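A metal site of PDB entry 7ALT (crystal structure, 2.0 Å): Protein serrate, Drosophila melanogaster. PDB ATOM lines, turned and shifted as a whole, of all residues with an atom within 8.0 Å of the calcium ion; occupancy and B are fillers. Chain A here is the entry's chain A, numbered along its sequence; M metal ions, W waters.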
ATOM      1  N   SER A  12      12.425 -18.052 -25.533  1.00  0.00           N
ATOM      2  CA  SER A  12      12.771 -16.639 -25.680  1.00  0.00           C
ATOM      3  C   SER A  12      11.592 -15.841 -25.135  1.00  0.00           C
ATOM      4  O   SER A  12      10.535 -15.777 -25.760  1.00  0.00           O
ATOM      5  CB  SER A  12      13.075 -16.281 -27.129  1.00  0.00           C
ATOM      6  OG  SER A  12      13.437 -14.916 -27.225  1.00  0.00           O
ATOM      7  N   ASN A  13      11.778 -15.284 -23.943  1.00  0.00           N
ATOM      8  CA  ASN A  13      10.819 -14.382 -23.296  1.00  0.00           C
ATOM      9  C   ASN A  13      11.609 -13.162 -22.838  1.00  0.00           C
ATOM     10  O   ASN A  13      11.897 -12.977 -21.649  1.00  0.00           O
ATOM     11  CB  ASN A  13      10.108 -15.087 -22.137  1.00  0.00           C
ATOM     12  CG  ASN A  13       9.094 -14.199 -21.447  1.00  0.00           C
ATOM     13  OD1 ASN A  13       8.838 -13.080 -21.877  1.00  0.00           O
ATOM     14  ND2 ASN A  13       8.518 -14.699 -20.352  1.00  0.00           N
ATOM     15  N   THR A  14      11.979 -12.303 -23.803  1.00  0.00           N
ATOM     16  CA  THR A  14      12.998 -11.290 -23.572  1.00  0.00           C
ATOM     17  C   THR A  14      12.588 -10.261 -22.526  1.00  0.00           C
ATOM     18  O   THR A  14      13.454  -9.718 -21.831  1.00  0.00           O
ATOM     19  CB  THR A  14      13.324 -10.578 -24.892  1.00  0.00           C
ATOM     20  OG1 THR A  14      12.100 -10.218 -25.552  1.00  0.00           O
ATOM     21  CG2 THR A  14      14.153 -11.467 -25.797  1.00  0.00           C
ATOM     22  N   ASN A  15      11.299  -9.973 -22.418  1.00  0.00           N
ATOM     23  CA  ASN A  15      10.820  -8.933 -21.513  1.00  0.00           C
ATOM     24  C   ASN A  15      10.305  -9.490 -20.181  1.00  0.00           C
ATOM     25  O   ASN A  15       9.751  -8.719 -19.387  1.00  0.00           O
ATOM     26  CB  ASN A  15       9.737  -8.100 -22.193  1.00  0.00           C
ATOM     27  CG  ASN A  15       8.509  -8.915 -22.574  1.00  0.00           C
ATOM     28  OD1 ASN A  15       8.371 -10.074 -22.195  1.00  0.00           O
ATOM     29  ND2 ASN A  15       7.597  -8.291 -23.312  1.00  0.00           N
ATOM     30  N   SER A  16      10.468 -10.787 -19.946  1.00  0.00           N
ATOM     31  CA  SER A  16      10.102 -11.430 -18.681  1.00  0.00           C
ATOM     32  C   SER A  16       8.649 -11.147 -18.314  1.00  0.00           C
ATOM     33  O   SER A  16       8.317 -10.840 -17.159  1.00  0.00           O
ATOM     34  CB  SER A  16      11.047 -11.009 -17.545  1.00  0.00           C
ATOM     35  OG  SER A  16      12.403 -11.161 -17.931  1.00  0.00           O
ATOM     36  N   HIS A  17       7.770 -11.271 -19.294  1.00  0.00           N
ATOM     37  CA  HIS A  17       6.338 -11.080 -19.099  1.00  0.00           C
ATOM     38  C   HIS A  17       5.622 -12.432 -18.972  1.00  0.00           C
ATOM     39  O   HIS A  17       6.148 -13.484 -19.311  1.00  0.00           O
ATOM     40  CB  HIS A  17       5.723 -10.315 -20.269  1.00  0.00           C
ATOM     41  CG  HIS A  17       5.848  -8.824 -20.171  1.00  0.00           C
ATOM     42  ND1 HIS A  17       6.943  -8.200 -19.615  1.00  0.00           N
ATOM     43  CD2 HIS A  17       5.017  -7.837 -20.582  1.00  0.00           C
ATOM     44  CE1 HIS A  17       6.784  -6.898 -19.680  1.00  0.00           C
ATOM     45  NE2 HIS A  17       5.622  -6.639 -20.254  1.00  0.00           N
ATOM     46  N   LEU A  18       4.376 -12.359 -18.509  1.00  0.00           N
ATOM     47  CA  LEU A  18       3.444 -13.473 -18.574  1.00  0.00           C
ATOM     48  C   LEU A  18       2.579 -13.353 -19.819  1.00  0.00           C
ATOM     49  O   LEU A  18       2.588 -12.325 -20.513  1.00  0.00           O
ATOM     50  CB  LEU A  18       2.573 -13.512 -17.317  1.00  0.00           C
ATOM     51  CG  LEU A  18       3.312 -13.667 -15.997  1.00  0.00           C
ATOM     52  CD1 LEU A  18       2.378 -13.339 -14.837  1.00  0.00           C
ATOM     53  CD2 LEU A  18       3.884 -15.074 -15.853  1.00  0.00           C
ATOM     54  N   LEU A  19       1.807 -14.396 -20.101  1.00  0.00           N
ATOM     55  CA  LEU A  19       0.937 -14.344 -21.280  1.00  0.00           C
ATOM     56  C   LEU A  19      -0.122 -13.255 -21.138  1.00  0.00           C
ATOM     57  O   LEU A  19      -0.482 -12.611 -22.132  1.00  0.00           O
ATOM     58  CB  LEU A  19       0.273 -15.700 -21.515  1.00  0.00           C
ATOM     59  CG  LEU A  19      -0.254 -15.956 -22.931  1.00  0.00           C
ATOM     60  CD1 LEU A  19       0.809 -15.737 -23.998  1.00  0.00           C
ATOM     61  CD2 LEU A  19      -0.816 -17.373 -23.029  1.00  0.00           C
ATOM     62  N   GLY A  21       0.275 -10.410 -20.026  1.00  0.00           N
ATOM     63  CA  GLY A  21       0.880  -9.110 -20.185  1.00  0.00           C
ATOM     64  C   GLY A  21       1.473  -8.518 -18.923  1.00  0.00           C
ATOM     65  O   GLY A  21       2.121  -7.461 -19.008  1.00  0.00           O
ATOM     66  N   TYR A  22       1.277  -9.139 -17.774  1.00  0.00           N
ATOM     67  CA  TYR A  22       1.895  -8.680 -16.549  1.00  0.00           C
ATOM     68  C   TYR A  22       3.323  -9.220 -16.457  1.00  0.00           C
ATOM     69  O   TYR A  22       3.789  -9.989 -17.309  1.00  0.00           O
ATOM     70  CB  TYR A  22       1.066  -9.096 -15.333  1.00  0.00           C
ATOM     71  CG  TYR A  22      -0.153  -8.233 -15.085  1.00  0.00           C
ATOM     72  CD1 TYR A  22      -0.086  -6.850 -15.195  1.00  0.00           C
ATOM     73  CD2 TYR A  22      -1.373  -8.801 -14.736  1.00  0.00           C
ATOM     74  CE1 TYR A  22      -1.200  -6.060 -14.972  1.00  0.00           C
ATOM     75  CE2 TYR A  22      -2.490  -8.023 -14.508  1.00  0.00           C
ATOM     76  CZ  TYR A  22      -2.399  -6.651 -14.628  1.00  0.00           C
ATOM     77  OH  TYR A  22      -3.512  -5.861 -14.404  1.00  0.00           O
ATOM     78  N   CYS A  24       6.560 -11.311 -14.745  1.00  0.00           N
ATOM     79  CA  CYS A  24       6.892 -12.455 -13.933  1.00  0.00           C
ATOM     80  C   CYS A  24       7.326 -12.000 -12.542  1.00  0.00           C
ATOM     81  O   CYS A  24       7.547 -10.815 -12.289  1.00  0.00           O
ATOM     82  CB  CYS A  24       7.994 -13.280 -14.580  1.00  0.00           C
ATOM     83  SG  CYS A  24       7.450 -14.259 -16.000  1.00  0.00           S
ATOM     84  N   CYS A  41      11.327 -14.370 -14.929  1.00  0.00           N
ATOM     85  CA  CYS A  41      10.521 -15.565 -14.773  1.00  0.00           C
ATOM     86  C   CYS A  41      11.374 -16.693 -14.187  1.00  0.00           C
ATOM     87  O   CYS A  41      12.614 -16.661 -14.224  1.00  0.00           O
ATOM     88  CB  CYS A  41       9.934 -15.991 -16.126  1.00  0.00           C
ATOM     89  SG  CYS A  41       9.158 -14.635 -17.029  1.00  0.00           S
ATOM     90  N   SER A  78      14.054 -16.188 -17.698  1.00  0.00           N
ATOM     91  CA  SER A  78      13.091 -15.768 -18.703  1.00  0.00           C
ATOM     92  C   SER A  78      13.416 -16.357 -20.072  1.00  0.00           C
ATOM     93  O   SER A  78      12.530 -16.887 -20.748  1.00  0.00           O
ATOM     94  CB  SER A  78      13.040 -14.240 -18.756  1.00  0.00           C
ATOM     95  OG  SER A  78      12.583 -13.714 -17.522  1.00  0.00           O
ATOM     96  N   SER A  79      14.683 -16.265 -20.484  1.00  0.00           N
ATOM     97  CA  SER A  79      15.126 -16.820 -21.761  1.00  0.00           C
ATOM     98  C   SER A  79      16.371 -17.674 -21.540  1.00  0.00           C
ATOM     99  O   SER A  79      17.251 -17.321 -20.758  1.00  0.00           O
ATOM    100  CB  SER A  79      15.443 -15.700 -22.765  1.00  0.00           C
ATOM    101  OG  SER A  79      14.410 -14.745 -22.797  1.00  0.00           O
ATOM    102  N   ILE A 123       3.161 -18.509 -18.885  1.00  0.00           N
ATOM    103  CA  ILE A 123       4.012 -17.680 -19.733  1.00  0.00           C
ATOM    104  C   ILE A 123       3.617 -17.843 -21.195  1.00  0.00           C
ATOM    105  O   ILE A 123       3.490 -16.856 -21.935  1.00  0.00           O
ATOM    106  CB  ILE A 123       5.489 -18.053 -19.524  1.00  0.00           C
ATOM    107  CG1 ILE A 123       5.975 -17.596 -18.149  1.00  0.00           C
ATOM    108  CG2 ILE A 123       6.346 -17.445 -20.618  1.00  0.00           C
ATOM    109  CD1 ILE A 123       7.182 -18.375 -17.674  1.00  0.00           C
ATOM    110  N   GLU A 124       3.452 -19.072 -21.651  1.00  0.00           N
ATOM    111  CA  GLU A 124       3.138 -19.306 -23.056  1.00  0.00           C
ATOM    112  C   GLU A 124       2.549 -20.703 -23.181  1.00  0.00           C
ATOM    113  O   GLU A 124       2.770 -21.566 -22.324  1.00  0.00           O
ATOM    114  CB  GLU A 124       4.378 -19.157 -23.932  1.00  0.00           C
ATOM    115  CG  GLU A 124       4.119 -19.136 -25.430  1.00  0.00           C
ATOM    116  CD  GLU A 124       3.128 -18.069 -25.837  1.00  0.00           C
ATOM    117  OE1 GLU A 124       3.555 -16.918 -26.063  1.00  0.00           O
ATOM    118  OE2 GLU A 124       1.924 -18.406 -25.959  1.00  0.00           O
ATOM    119  N   GLY A 145       4.966 -17.605 -30.229  1.00  0.00           N
ATOM    120  CA  GLY A 145       3.748 -17.120 -29.608  1.00  0.00           C
ATOM    121  C   GLY A 145       3.733 -15.604 -29.433  1.00  0.00           C
ATOM    122  O   GLY A 145       4.687 -14.895 -29.761  1.00  0.00           O
ATOM    123  N   ARG A 146       2.618 -15.118 -28.888  1.00  0.00           N
ATOM    124  CA  ARG A 146       2.468 -13.685 -28.645  1.00  0.00           C
ATOM    125  C   ARG A 146       3.489 -13.198 -27.624  1.00  0.00           C
ATOM    126  O   ARG A 146       3.980 -12.059 -27.718  1.00  0.00           O
ATOM    127  CB  ARG A 146       1.050 -13.384 -28.151  1.00  0.00           C
ATOM    128  CG  ARG A 146       0.014 -13.208 -29.265  1.00  0.00           C
ATOM    129  CD  ARG A 146      -1.205 -12.408 -28.781  1.00  0.00           C
ATOM    130  NE  ARG A 146      -1.393 -11.174 -29.541  1.00  0.00           N
ATOM    131  CZ  ARG A 146      -1.576  -9.972 -29.015  1.00  0.00           C
ATOM    132  NH1 ARG A 146      -1.613  -9.791 -27.703  1.00  0.00           N
ATOM    133  NH2 ARG A 146      -1.719  -8.928 -29.819  1.00  0.00           N
ATOM    134  N   ASN A 147       3.798 -14.018 -26.616  1.00  0.00           N
ATOM    135  CA  ASN A 147       4.680 -13.626 -25.522  1.00  0.00           C
ATOM    136  C   ASN A 147       6.064 -14.256 -25.603  1.00  0.00           C
ATOM    137  O   ASN A 147       7.067 -13.549 -25.436  1.00  0.00           O
ATOM    138  CB  ASN A 147       4.029 -14.003 -24.177  1.00  0.00           C
ATOM    139  CG  ASN A 147       4.812 -13.467 -22.976  1.00  0.00           C
ATOM    140  OD1 ASN A 147       5.095 -12.278 -22.883  1.00  0.00           O
ATOM    141  ND2 ASN A 147       5.164 -14.358 -22.053  1.00  0.00           N
ATOM    142  N   ALA A 148       6.150 -15.563 -25.799  1.00  0.00           N
ATOM    143  CA  ALA A 148       7.442 -16.235 -25.834  1.00  0.00           C
ATOM    144  C   ALA A 148       7.532 -17.139 -27.057  1.00  0.00           C
ATOM    145  O   ALA A 148       6.521 -17.581 -27.611  1.00  0.00           O
ATOM    146  CB  ALA A 148       7.687 -17.048 -24.564  1.00  0.00           C
ATOM    147  N   ARG A 149       8.761 -17.394 -27.478  1.00  0.00           N
ATOM    148  CA  ARG A 149       9.062 -18.396 -28.497  1.00  0.00           C
ATOM    149  C   ARG A 149       9.614 -19.628 -27.799  1.00  0.00           C
ATOM    150  O   ARG A 149      10.593 -19.538 -27.047  1.00  0.00           O
ATOM    151  CB  ARG A 149      10.058 -17.855 -29.519  1.00  0.00           C
ATOM    152  CG  ARG A 149      10.411 -18.835 -30.641  1.00  0.00           C
ATOM    153  CD  ARG A 149      11.679 -18.395 -31.385  1.00  0.00           C
ATOM    154  NE  ARG A 149      11.916 -19.176 -32.589  1.00  0.00           N
ATOM    155  CZ  ARG A 149      12.546 -18.728 -33.676  1.00  0.00           C
ATOM    156  NH1 ARG A 149      13.114 -17.542 -33.695  1.00  0.00           N
ATOM    157  NH2 ARG A 149      12.613 -19.498 -34.760  1.00  0.00           N
HETATM  158 CA    CA M   1       7.421 -11.911 -23.567  1.00  0.00          CA
HETATM  159  O   HOH W   1       9.345 -11.123 -25.490  1.00  0.00           O
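SG of Cys 24 is disulfide-bonded to SG of Cys 41 (2.0 Å).
The side-chain amide nitrogen (ND2) of Asn 147 lies within hydrogen-bond range of the backbone carbonyl oxygen (O) of His 17 (3.0 Å).
OD1 of Asn 13 lies close to N of Ser 16 (3.4 Å).
ND2 of Asn 13 sits at hydrogen-bond distance from SG of Cys 41 (3.4 Å).
OD1 of Asn 147 lies close to O of Leu 18.
N of Asn 147 lies within hydrogen-bond range of OE1 of Glu 124.
The side-chain amide nitrogen (ND2) of Asn 147 lies within hydrogen-bond range of the backbone carbonyl oxygen (O) of Ile 123 (3.0 Å).
The backbone carbonyl oxygen (O) of Asn 15 lies within hydrogen-bond range of a ring nitrogen (ND1) of His 17 (2.9 Å).
The nearest printed residue that does not touch the calcium ion is His 17 (4.04 Å).
The calcium ion is bound by OD1 of Asn 147, OD1 of Asn 15, OD1 of Asn 13, O of Asn 147 and water W1.
The calcium ion has five donor atoms within binding distance.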
